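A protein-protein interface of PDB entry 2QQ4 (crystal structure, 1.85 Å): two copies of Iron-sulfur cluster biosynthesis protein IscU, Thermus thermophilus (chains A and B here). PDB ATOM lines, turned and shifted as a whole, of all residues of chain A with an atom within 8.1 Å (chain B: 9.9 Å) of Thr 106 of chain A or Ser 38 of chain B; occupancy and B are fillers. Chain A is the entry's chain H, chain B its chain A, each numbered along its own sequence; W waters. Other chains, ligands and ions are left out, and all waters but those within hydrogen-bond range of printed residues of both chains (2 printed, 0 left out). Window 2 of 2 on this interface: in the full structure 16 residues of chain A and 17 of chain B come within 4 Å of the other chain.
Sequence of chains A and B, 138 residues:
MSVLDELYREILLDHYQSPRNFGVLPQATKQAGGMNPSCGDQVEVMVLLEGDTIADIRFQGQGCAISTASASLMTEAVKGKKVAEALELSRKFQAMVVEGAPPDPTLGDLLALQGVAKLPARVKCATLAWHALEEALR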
ATOM      1  N   ALA A  77      -8.227   5.023   2.651  1.00  0.00           N
ATOM      2  CA  ALA A  77      -9.328   5.443   3.506  1.00  0.00           C
ATOM      3  C   ALA A  77     -10.118   6.646   3.006  1.00  0.00           C
ATOM      4  O   ALA A  77     -11.303   6.774   3.323  1.00  0.00           O
ATOM      5  CB  ALA A  77      -8.816   5.716   4.918  1.00  0.00           C
ATOM      6  N   LYS A  81     -14.190   9.617  -1.149  1.00  0.00           N
ATOM      7  CA  LYS A  81     -14.942  10.199  -0.043  1.00  0.00           C
ATOM      8  C   LYS A  81     -15.140  11.692  -0.257  1.00  0.00           C
ATOM      9  O   LYS A  81     -14.524  12.286  -1.144  1.00  0.00           O
ATOM     10  CB  LYS A  81     -14.201   9.986   1.277  1.00  0.00           C
ATOM     11  CG  LYS A  81     -14.024   8.539   1.678  1.00  0.00           C
ATOM     12  CD  LYS A  81     -15.345   7.900   2.042  1.00  0.00           C
ATOM     13  CE  LYS A  81     -15.149   6.459   2.478  1.00  0.00           C
ATOM     14  NZ  LYS A  81     -16.445   5.806   2.809  1.00  0.00           N
ATOM     15  N   GLU A  85     -15.642  14.606   4.731  1.00  0.00           N
ATOM     16  CA  GLU A  85     -15.521  13.285   5.346  1.00  0.00           C
ATOM     17  C   GLU A  85     -14.053  12.940   5.583  1.00  0.00           C
ATOM     18  O   GLU A  85     -13.666  12.527   6.677  1.00  0.00           O
ATOM     19  CB  GLU A  85     -16.138  12.206   4.450  1.00  0.00           C
ATOM     20  CG  GLU A  85     -17.643  12.289   4.272  1.00  0.00           C
ATOM     21  CD  GLU A  85     -18.185  11.147   3.427  1.00  0.00           C
ATOM     22  OE1 GLU A  85     -17.803  11.040   2.242  1.00  0.00           O
ATOM     23  OE2 GLU A  85     -18.989  10.350   3.953  1.00  0.00           O
ATOM     24  N   GLU A  88     -12.778  14.611   8.354  1.00  0.00           N
ATOM     25  CA  GLU A  88     -13.346  14.066   9.581  1.00  0.00           C
ATOM     26  C   GLU A  88     -12.531  12.845  10.005  1.00  0.00           C
ATOM     27  O   GLU A  88     -12.214  12.669  11.181  1.00  0.00           O
ATOM     28  CB  GLU A  88     -14.808  13.674   9.355  1.00  0.00           C
ATOM     29  CG  GLU A  88     -15.532  13.234  10.615  1.00  0.00           C
ATOM     30  CD  GLU A  88     -15.321  14.199  11.769  1.00  0.00           C
ATOM     31  OE1 GLU A  88     -15.437  15.425  11.556  1.00  0.00           O
ATOM     32  OE2 GLU A  88     -15.044  13.729  12.891  1.00  0.00           O
ATOM     33  N   LEU A  89     -12.191  12.004   9.034  1.00  0.00           N
ATOM     34  CA  LEU A  89     -11.393  10.815   9.300  1.00  0.00           C
ATOM     35  C   LEU A  89     -10.022  11.233   9.817  1.00  0.00           C
ATOM     36  O   LEU A  89      -9.452  10.581  10.690  1.00  0.00           O
ATOM     37  CB  LEU A  89     -11.230   9.990   8.024  1.00  0.00           C
ATOM     38  CG  LEU A  89     -12.055   8.703   7.937  1.00  0.00           C
ATOM     39  CD1 LEU A  89     -12.049   8.171   6.514  1.00  0.00           C
ATOM     40  CD2 LEU A  89     -11.482   7.681   8.895  1.00  0.00           C
ATOM     41  N   LYS A  92     -10.411  12.184  13.501  1.00  0.00           N
ATOM     42  CA  LYS A  92     -10.470  10.983  14.324  1.00  0.00           C
ATOM     43  C   LYS A  92      -9.124  10.273  14.382  1.00  0.00           C
ATOM     44  O   LYS A  92      -8.724   9.779  15.433  1.00  0.00           O
ATOM     45  CB  LYS A  92     -11.512  10.009  13.771  1.00  0.00           C
ATOM     46  CG  LYS A  92     -12.904  10.585  13.602  1.00  0.00           C
ATOM     47  CD  LYS A  92     -13.812   9.559  12.938  1.00  0.00           C
ATOM     48  CE  LYS A  92     -15.171  10.144  12.591  1.00  0.00           C
ATOM     49  NZ  LYS A  92     -16.006   9.169  11.831  1.00  0.00           N
ATOM     50  N   PHE A  93      -8.429  10.214  13.251  1.00  0.00           N
ATOM     51  CA  PHE A  93      -7.137   9.539  13.204  1.00  0.00           C
ATOM     52  C   PHE A  93      -6.113  10.217  14.104  1.00  0.00           C
ATOM     53  O   PHE A  93      -5.421   9.558  14.880  1.00  0.00           O
ATOM     54  CB  PHE A  93      -6.594   9.504  11.777  1.00  0.00           C
ATOM     55  CG  PHE A  93      -5.270   8.802  11.656  1.00  0.00           C
ATOM     56  CD1 PHE A  93      -5.193   7.414  11.754  1.00  0.00           C
ATOM     57  CD2 PHE A  93      -4.099   9.525  11.478  1.00  0.00           C
ATOM     58  CE1 PHE A  93      -3.965   6.758  11.676  1.00  0.00           C
ATOM     59  CE2 PHE A  93      -2.864   8.879  11.400  1.00  0.00           C
ATOM     60  CZ  PHE A  93      -2.798   7.496  11.500  1.00  0.00           C
ATOM     61  N   PRO A 103     -10.391   5.041  19.750  1.00  0.00           N
ATOM     62  CA  PRO A 103     -10.681   5.055  18.315  1.00  0.00           C
ATOM     63  C   PRO A 103     -11.902   4.226  17.939  1.00  0.00           C
ATOM     64  O   PRO A 103     -11.997   3.052  18.297  1.00  0.00           O
ATOM     65  CB  PRO A 103      -9.404   4.492  17.714  1.00  0.00           C
ATOM     66  CG  PRO A 103      -9.036   3.443  18.714  1.00  0.00           C
ATOM     67  CD  PRO A 103      -9.254   4.150  20.043  1.00  0.00           C
ATOM     68  N   ASP A 104     -12.837   4.841  17.221  1.00  0.00           N
ATOM     69  CA  ASP A 104     -14.035   4.131  16.797  1.00  0.00           C
ATOM     70  C   ASP A 104     -13.654   3.192  15.656  1.00  0.00           C
ATOM     71  O   ASP A 104     -12.584   3.333  15.060  1.00  0.00           O
ATOM     72  CB  ASP A 104     -15.113   5.119  16.333  1.00  0.00           C
ATOM     73  CG  ASP A 104     -14.640   6.010  15.208  1.00  0.00           C
ATOM     74  OD1 ASP A 104     -14.127   5.475  14.205  1.00  0.00           O
ATOM     75  OD2 ASP A 104     -14.786   7.245  15.321  1.00  0.00           O
ATOM     76  N   PRO A 105     -14.519   2.214  15.343  1.00  0.00           N
ATOM     77  CA  PRO A 105     -14.225   1.272  14.261  1.00  0.00           C
ATOM     78  C   PRO A 105     -14.261   1.912  12.876  1.00  0.00           C
ATOM     79  O   PRO A 105     -13.824   1.305  11.900  1.00  0.00           O
ATOM     80  CB  PRO A 105     -15.305   0.210  14.435  1.00  0.00           C
ATOM     81  CG  PRO A 105     -16.466   1.009  14.931  1.00  0.00           C
ATOM     82  CD  PRO A 105     -15.816   1.898  15.969  1.00  0.00           C
ATOM     83  N   THR A 106     -14.777   3.138  12.796  1.00  0.00           N
ATOM     84  CA  THR A 106     -14.874   3.841  11.520  1.00  0.00           C
ATOM     85  C   THR A 106     -13.497   4.199  10.972  1.00  0.00           C
ATOM     86  O   THR A 106     -13.386   4.847   9.932  1.00  0.00           O
ATOM     87  CB  THR A 106     -15.704   5.137  11.640  1.00  0.00           C
ATOM     88  OG1 THR A 106     -14.849   6.228  12.000  1.00  0.00           O
ATOM     89  CG2 THR A 106     -16.775   4.978  12.703  1.00  0.00           C
ATOM     90  N   LEU A 107     -12.456   3.794  11.687  1.00  0.00           N
ATOM     91  CA  LEU A 107     -11.089   4.042  11.249  1.00  0.00           C
ATOM     92  C   LEU A 107     -10.620   2.808  10.501  1.00  0.00           C
ATOM     93  O   LEU A 107      -9.641   2.851   9.760  1.00  0.00           O
ATOM     94  CB  LEU A 107     -10.175   4.309  12.446  1.00  0.00           C
ATOM     95  CG  LEU A 107     -10.211   5.737  12.993  1.00  0.00           C
ATOM     96  CD1 LEU A 107      -9.339   5.845  14.230  1.00  0.00           C
ATOM     97  CD2 LEU A 107      -9.730   6.702  11.915  1.00  0.00           C
ATOM     98  N   GLY A 108     -11.334   1.703  10.717  1.00  0.00           N
ATOM     99  CA  GLY A 108     -11.017   0.454  10.050  1.00  0.00           C
ATOM    100  C   GLY A 108      -9.576   0.005  10.147  1.00  0.00           C
ATOM    101  O   GLY A 108      -9.022  -0.107  11.239  1.00  0.00           O
ATOM    102  N   ASP A 109      -8.969  -0.262   8.998  1.00  0.00           N
ATOM    103  CA  ASP A 109      -7.591  -0.716   8.964  1.00  0.00           C
ATOM    104  C   ASP A 109      -6.629   0.294   9.575  1.00  0.00           C
ATOM    105  O   ASP A 109      -5.534  -0.069   9.989  1.00  0.00           O
ATOM    106  CB  ASP A 109      -7.179  -1.045   7.530  1.00  0.00           C
ATOM    107  CG  ASP A 109      -7.887  -2.280   6.993  1.00  0.00           C
ATOM    108  OD1 ASP A 109      -8.522  -2.997   7.799  1.00  0.00           O
ATOM    109  OD2 ASP A 109      -7.801  -2.537   5.774  1.00  0.00           O
ATOM    110  N   LEU A 110      -7.034   1.559   9.633  1.00  0.00           N
ATOM    111  CA  LEU A 110      -6.182   2.590  10.221  1.00  0.00           C
ATOM    112  C   LEU A 110      -5.917   2.279  11.696  1.00  0.00           C
ATOM    113  O   LEU A 110      -4.942   2.753  12.277  1.00  0.00           O
ATOM    114  CB  LEU A 110      -6.837   3.970  10.083  1.00  0.00           C
ATOM    115  CG  LEU A 110      -6.911   4.542   8.661  1.00  0.00           C
ATOM    116  CD1 LEU A 110      -7.783   5.796   8.643  1.00  0.00           C
ATOM    117  CD2 LEU A 110      -5.514   4.848   8.161  1.00  0.00           C
ATOM    118  N   LEU A 111      -6.784   1.475  12.305  1.00  0.00           N
ATOM    119  CA  LEU A 111      -6.603   1.119  13.705  1.00  0.00           C
ATOM    120  C   LEU A 111      -5.253   0.431  13.923  1.00  0.00           C
ATOM    121  O   LEU A 111      -4.753   0.369  15.044  1.00  0.00           O
ATOM    122  CB  LEU A 111      -7.746   0.215  14.174  1.00  0.00           C
ATOM    123  CG  LEU A 111      -9.113   0.907  14.252  1.00  0.00           C
ATOM    124  CD1 LEU A 111     -10.169  -0.070  14.755  1.00  0.00           C
ATOM    125  CD2 LEU A 111      -9.018   2.106  15.186  1.00  0.00           C
ATOM    126  N   GLY B  34     -25.967  -5.840   3.891  1.00  0.00           N
ATOM    127  CA  GLY B  34     -25.818  -5.366   5.246  1.00  0.00           C
ATOM    128  C   GLY B  34     -24.855  -4.205   5.209  1.00  0.00           C
ATOM    129  O   GLY B  34     -23.978  -4.143   4.345  1.00  0.00           O
ATOM    130  N   MET B  35     -25.008  -3.274   6.139  1.00  0.00           N
ATOM    131  CA  MET B  35     -24.123  -2.132   6.162  1.00  0.00           C
ATOM    132  C   MET B  35     -23.830  -1.623   7.569  1.00  0.00           C
ATOM    133  O   MET B  35     -24.712  -1.589   8.432  1.00  0.00           O
ATOM    134  CB  MET B  35     -24.731  -1.013   5.317  1.00  0.00           C
ATOM    135  CG  MET B  35     -23.776   0.098   4.958  1.00  0.00           C
ATOM    136  SD  MET B  35     -24.536   1.236   3.782  1.00  0.00           S
ATOM    137  CE  MET B  35     -24.473   0.250   2.277  1.00  0.00           C
ATOM    138  N   ASN B  36     -22.570  -1.257   7.790  1.00  0.00           N
ATOM    139  CA  ASN B  36     -22.112  -0.686   9.055  1.00  0.00           C
ATOM    140  C   ASN B  36     -22.037   0.784   8.650  1.00  0.00           C
ATOM    141  O   ASN B  36     -21.016   1.233   8.129  1.00  0.00           O
ATOM    142  CB  ASN B  36     -20.717  -1.209   9.427  1.00  0.00           C
ATOM    143  CG  ASN B  36     -20.756  -2.532  10.179  1.00  0.00           C
ATOM    144  OD1 ASN B  36     -19.732  -3.206  10.324  1.00  0.00           O
ATOM    145  ND2 ASN B  36     -21.930  -2.901  10.676  1.00  0.00           N
ATOM    146  N   PRO B  37     -23.124   1.545   8.872  1.00  0.00           N
ATOM    147  CA  PRO B  37     -23.202   2.968   8.521  1.00  0.00           C
ATOM    148  C   PRO B  37     -21.962   3.815   8.804  1.00  0.00           C
ATOM    149  O   PRO B  37     -21.624   4.703   8.020  1.00  0.00           O
ATOM    150  CB  PRO B  37     -24.420   3.434   9.315  1.00  0.00           C
ATOM    151  CG  PRO B  37     -25.326   2.247   9.240  1.00  0.00           C
ATOM    152  CD  PRO B  37     -24.363   1.109   9.538  1.00  0.00           C
ATOM    153  N   SER B  38     -21.280   3.541   9.912  1.00  0.00           N
ATOM    154  CA  SER B  38     -20.099   4.318  10.269  1.00  0.00           C
ATOM    155  C   SER B  38     -18.781   3.772   9.717  1.00  0.00           C
ATOM    156  O   SER B  38     -18.117   4.447   8.928  1.00  0.00           O
ATOM    157  CB  SER B  38     -20.009   4.458  11.793  1.00  0.00           C
ATOM    158  OG  SER B  38     -20.025   3.198  12.437  1.00  0.00           O
ATOM    159  N   CYS B  39     -18.400   2.564  10.131  1.00  0.00           N
ATOM    160  CA  CYS B  39     -17.147   1.968   9.667  1.00  0.00           C
ATOM    161  C   CYS B  39     -17.067   1.977   8.147  1.00  0.00           C
ATOM    162  O   CYS B  39     -15.977   1.933   7.574  1.00  0.00           O
ATOM    163  CB  CYS B  39     -16.999   0.527  10.177  1.00  0.00           C
ATOM    164  SG  CYS B  39     -15.363  -0.239   9.865  1.00  0.00           S
ATOM    165  N   GLY B  40     -18.223   2.042   7.495  1.00  0.00           N
ATOM    166  CA  GLY B  40     -18.244   2.060   6.045  1.00  0.00           C
ATOM    167  C   GLY B  40     -18.206   0.675   5.432  1.00  0.00           C
ATOM    168  O   GLY B  40     -18.105   0.537   4.213  1.00  0.00           O
ATOM    169  N   ASP B  41     -18.278  -0.359   6.262  1.00  0.00           N
ATOM    170  CA  ASP B  41     -18.261  -1.712   5.734  1.00  0.00           C
ATOM    171  C   ASP B  41     -19.621  -2.011   5.122  1.00  0.00           C
ATOM    172  O   ASP B  41     -20.660  -1.634   5.666  1.00  0.00           O
ATOM    173  CB  ASP B  41     -17.992  -2.755   6.822  1.00  0.00           C
ATOM    174  CG  ASP B  41     -16.739  -2.470   7.630  1.00  0.00           C
ATOM    175  OD1 ASP B  41     -15.742  -1.964   7.074  1.00  0.00           O
ATOM    176  OD2 ASP B  41     -16.754  -2.785   8.836  1.00  0.00           O
ATOM    177  N   GLN B  42     -19.601  -2.679   3.979  1.00  0.00           N
ATOM    178  CA  GLN B  42     -20.825  -3.060   3.303  1.00  0.00           C
ATOM    179  C   GLN B  42     -20.625  -4.461   2.758  1.00  0.00           C
ATOM    180  O   GLN B  42     -19.542  -4.820   2.301  1.00  0.00           O
ATOM    181  CB  GLN B  42     -21.146  -2.087   2.169  1.00  0.00           C
ATOM    182  CG  GLN B  42     -20.094  -2.022   1.083  1.00  0.00           C
ATOM    183  CD  GLN B  42     -20.507  -1.117  -0.065  1.00  0.00           C
ATOM    184  OE1 GLN B  42     -19.773  -0.961  -1.040  1.00  0.00           O
ATOM    185  NE2 GLN B  42     -21.688  -0.515   0.047  1.00  0.00           N
ATOM    186  N   GLN B  62     -16.990  -4.168   0.411  1.00  0.00           N
ATOM    187  CA  GLN B  62     -15.719  -3.522   0.663  1.00  0.00           C
ATOM    188  C   GLN B  62     -15.779  -3.173   2.136  1.00  0.00           C
ATOM    189  O   GLN B  62     -16.861  -3.028   2.703  1.00  0.00           O
ATOM    190  CB  GLN B  62     -15.606  -2.228  -0.143  1.00  0.00           C
ATOM    191  CG  GLN B  62     -16.059  -2.324  -1.590  1.00  0.00           C
ATOM    192  CD  GLN B  62     -14.934  -2.669  -2.540  1.00  0.00           C
ATOM    193  OE1 GLN B  62     -14.345  -3.746  -2.462  1.00  0.00           O
ATOM    194  NE2 GLN B  62     -14.626  -1.748  -3.448  1.00  0.00           N
ATOM    195  N   GLY B  63     -14.622  -3.020   2.756  1.00  0.00           N
ATOM    196  CA  GLY B  63     -14.606  -2.681   4.162  1.00  0.00           C
ATOM    197  C   GLY B  63     -13.269  -3.009   4.776  1.00  0.00           C
ATOM    198  O   GLY B  63     -12.290  -3.265   4.064  1.00  0.00           O
ATOM    199  N   CYS B  64     -13.239  -3.009   6.101  1.00  0.00           N
ATOM    200  CA  CYS B  64     -12.025  -3.290   6.850  1.00  0.00           C
ATOM    201  C   CYS B  64     -11.640  -4.761   6.736  1.00  0.00           C
ATOM    202  O   CYS B  64     -12.461  -5.612   6.375  1.00  0.00           O
ATOM    203  CB  CYS B  64     -12.237  -2.933   8.312  1.00  0.00           C
ATOM    204  SG  CYS B  64     -13.363  -4.062   9.155  1.00  0.00           S
ATOM    205  N   ALA B 121     -16.390  -2.431  20.203  1.00  0.00           N
ATOM    206  CA  ALA B 121     -16.685  -1.547  19.079  1.00  0.00           C
ATOM    207  C   ALA B 121     -16.421  -2.144  17.696  1.00  0.00           C
ATOM    208  O   ALA B 121     -16.973  -1.672  16.708  1.00  0.00           O
ATOM    209  CB  ALA B 121     -15.919  -0.240  19.240  1.00  0.00           C
ATOM    210  N   ARG B 122     -15.595  -3.182  17.617  1.00  0.00           N
ATOM    211  CA  ARG B 122     -15.297  -3.805  16.323  1.00  0.00           C
ATOM    212  C   ARG B 122     -16.107  -5.090  16.079  1.00  0.00           C
ATOM    213  O   ARG B 122     -16.027  -5.708  15.010  1.00  0.00           O
ATOM    214  CB  ARG B 122     -13.796  -4.118  16.233  1.00  0.00           C
ATOM    215  CG  ARG B 122     -12.891  -2.896  16.383  1.00  0.00           C
ATOM    216  CD  ARG B 122     -11.451  -3.334  16.631  1.00  0.00           C
ATOM    217  NE  ARG B 122     -10.544  -2.237  16.976  1.00  0.00           N
ATOM    218  CZ  ARG B 122     -10.668  -1.453  18.046  1.00  0.00           C
ATOM    219  NH1 ARG B 122     -11.671  -1.628  18.898  1.00  0.00           N
ATOM    220  NH2 ARG B 122      -9.775  -0.498  18.273  1.00  0.00           N
ATOM    221  N   VAL B 123     -16.889  -5.494  17.070  1.00  0.00           N
ATOM    222  CA  VAL B 123     -17.686  -6.702  16.928  1.00  0.00           C
ATOM    223  C   VAL B 123     -18.617  -6.617  15.709  1.00  0.00           C
ATOM    224  O   VAL B 123     -18.853  -7.619  15.041  1.00  0.00           O
ATOM    225  CB  VAL B 123     -18.502  -6.983  18.226  1.00  0.00           C
ATOM    226  CG1 VAL B 123     -19.580  -8.049  17.971  1.00  0.00           C
ATOM    227  CG2 VAL B 123     -17.553  -7.472  19.327  1.00  0.00           C
ATOM    228  N   LYS B 124     -19.127  -5.425  15.409  1.00  0.00           N
ATOM    229  CA  LYS B 124     -20.022  -5.263  14.254  1.00  0.00           C
ATOM    230  C   LYS B 124     -19.323  -5.564  12.931  1.00  0.00           C
ATOM    231  O   LYS B 124     -19.968  -5.942  11.950  1.00  0.00           O
ATOM    232  CB  LYS B 124     -20.596  -3.846  14.205  1.00  0.00           C
ATOM    233  CG  LYS B 124     -19.546  -2.750  14.177  1.00  0.00           C
ATOM    234  CD  LYS B 124     -20.193  -1.358  14.137  1.00  0.00           C
ATOM    235  CE  LYS B 124     -19.574  -0.408  15.166  1.00  0.00           C
ATOM    236  NZ  LYS B 124     -19.914  -0.726  16.614  1.00  0.00           N
ATOM    237  N   CYS B 125     -18.002  -5.383  12.891  1.00  0.00           N
ATOM    238  CA  CYS B 125     -17.268  -5.670  11.668  1.00  0.00           C
ATOM    239  C   CYS B 125     -17.269  -7.174  11.415  1.00  0.00           C
ATOM    240  O   CYS B 125     -17.270  -7.623  10.260  1.00  0.00           O
ATOM    241  CB  CYS B 125     -15.833  -5.148  11.786  1.00  0.00           C
ATOM    242  SG  CYS B 125     -15.742  -3.380  12.098  1.00  0.00           S
ATOM    243  N   LEU B 128     -21.349  -8.403  10.657  1.00  0.00           N
ATOM    244  CA  LEU B 128     -22.027  -7.884   9.467  1.00  0.00           C
ATOM    245  C   LEU B 128     -22.403  -8.957   8.451  1.00  0.00           C
ATOM    246  O   LEU B 128     -23.571  -9.072   8.057  1.00  0.00           O
ATOM    247  CB  LEU B 128     -21.163  -6.810   8.793  1.00  0.00           C
ATOM    248  CG  LEU B 128     -21.798  -6.113   7.580  1.00  0.00           C
ATOM    249  CD1 LEU B 128     -23.107  -5.494   8.004  1.00  0.00           C
ATOM    250  CD2 LEU B 128     -20.866  -5.039   7.030  1.00  0.00           C
HETATM  251  O   HOH W   1     -16.866   3.097   2.969  1.00  0.00           O
HETATM  252  O   HOH W   2      -9.227  -3.831   4.122  1.00  0.00           O
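The side-chain sulfur (SG) of Cys 39 of chain B sits close to the backbone carbonyl oxygen (O) of Pro 105 of chain A, at 3.0 Å.
The side-chain amide oxygen of Asn 36 of chain B lies close to the backbone carbonyl oxygen of Lys 124 of chain B.
NZ of Lys 124 of chain B sits at hydrogen-bond distance from O of Ala 121 of chain B (3.1 Å).
The side-chain sulfur of Cys 125 of chain B sits close to the backbone carbonyl oxygen of Arg 122 of chain B, at 3.7 Å.
OG1 of Thr 106 of chain A lies within hydrogen-bond range of NZ of Lys 92 of chain A.
The side-chain hydroxyl (OG1) of Thr 106 of chain A lies within hydrogen-bond range of the side-chain carboxylate (OD1) of Asp 104 of chain A, 2.4 Å away.
Among the printed residues, merely in contact across the chains: Pro 105 of chain A with Ala 121 of chain B (3.3 Å), Pro 105 of chain A with Lys 124 of chain B (3.4 Å), Thr 106 of chain A with Ser 38 of chain B (3.4 Å), Thr 106 of chain A with Cys 39 of chain B (3.5 Å), Gly 108 of chain A with Cys 64 of chain B (3.998 Å), Asp 109 of chain A with Cys 64 of chain B (3.6 Å) and Leu 111 of chain A with Arg 122 of chain B (3.1 Å).
Ser 38 of chain B touches just one residue of chain A: Thr 106.
Pro 105 of chain A touches just these residues of chain B: Cys 39 (3.0 Å), Ala 121 (3.3 Å) and Lys 124 (3.4 Å).
Leu 107 of chain A touches none of the printed residues of chain B.
Of the printed residues of chain A, Ala 121 of chain B touches Pro 105 (3.3 Å).
Printed residues of chain B within 4 Å of Leu 111 of chain A: Arg 122 (3.1 Å).
Leu 110 of chain A touches none of the printed residues of chain B.
Glu 85 of chain A touches none of the printed residues of chain B.
The nearest residue of chain B that does not touch Thr 106 of chain A is Gly 40 of chain B (5.5 Å).
The nearest printed residue of chain B that does not touch Leu 111 of chain A is Cys 125 of chain B (7.0 Å).
Among the printed residues, no Asp or Glu carboxylate lies within 4 Å of a Lys or Arg side-chain nitrogen of the other chain.
No position is printed for both chains.
Water W2 lies within hydrogen-bond range of OD2 of Asp 109 of chain A and O of Gly 63 of chain B.
Water W1 lies within hydrogen-bond range of the side-chain amino group of Lys 81 of chain A (2.7 Å) and the backbone carbonyl oxygen of Gly 40 of chain B (3.1 Å).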
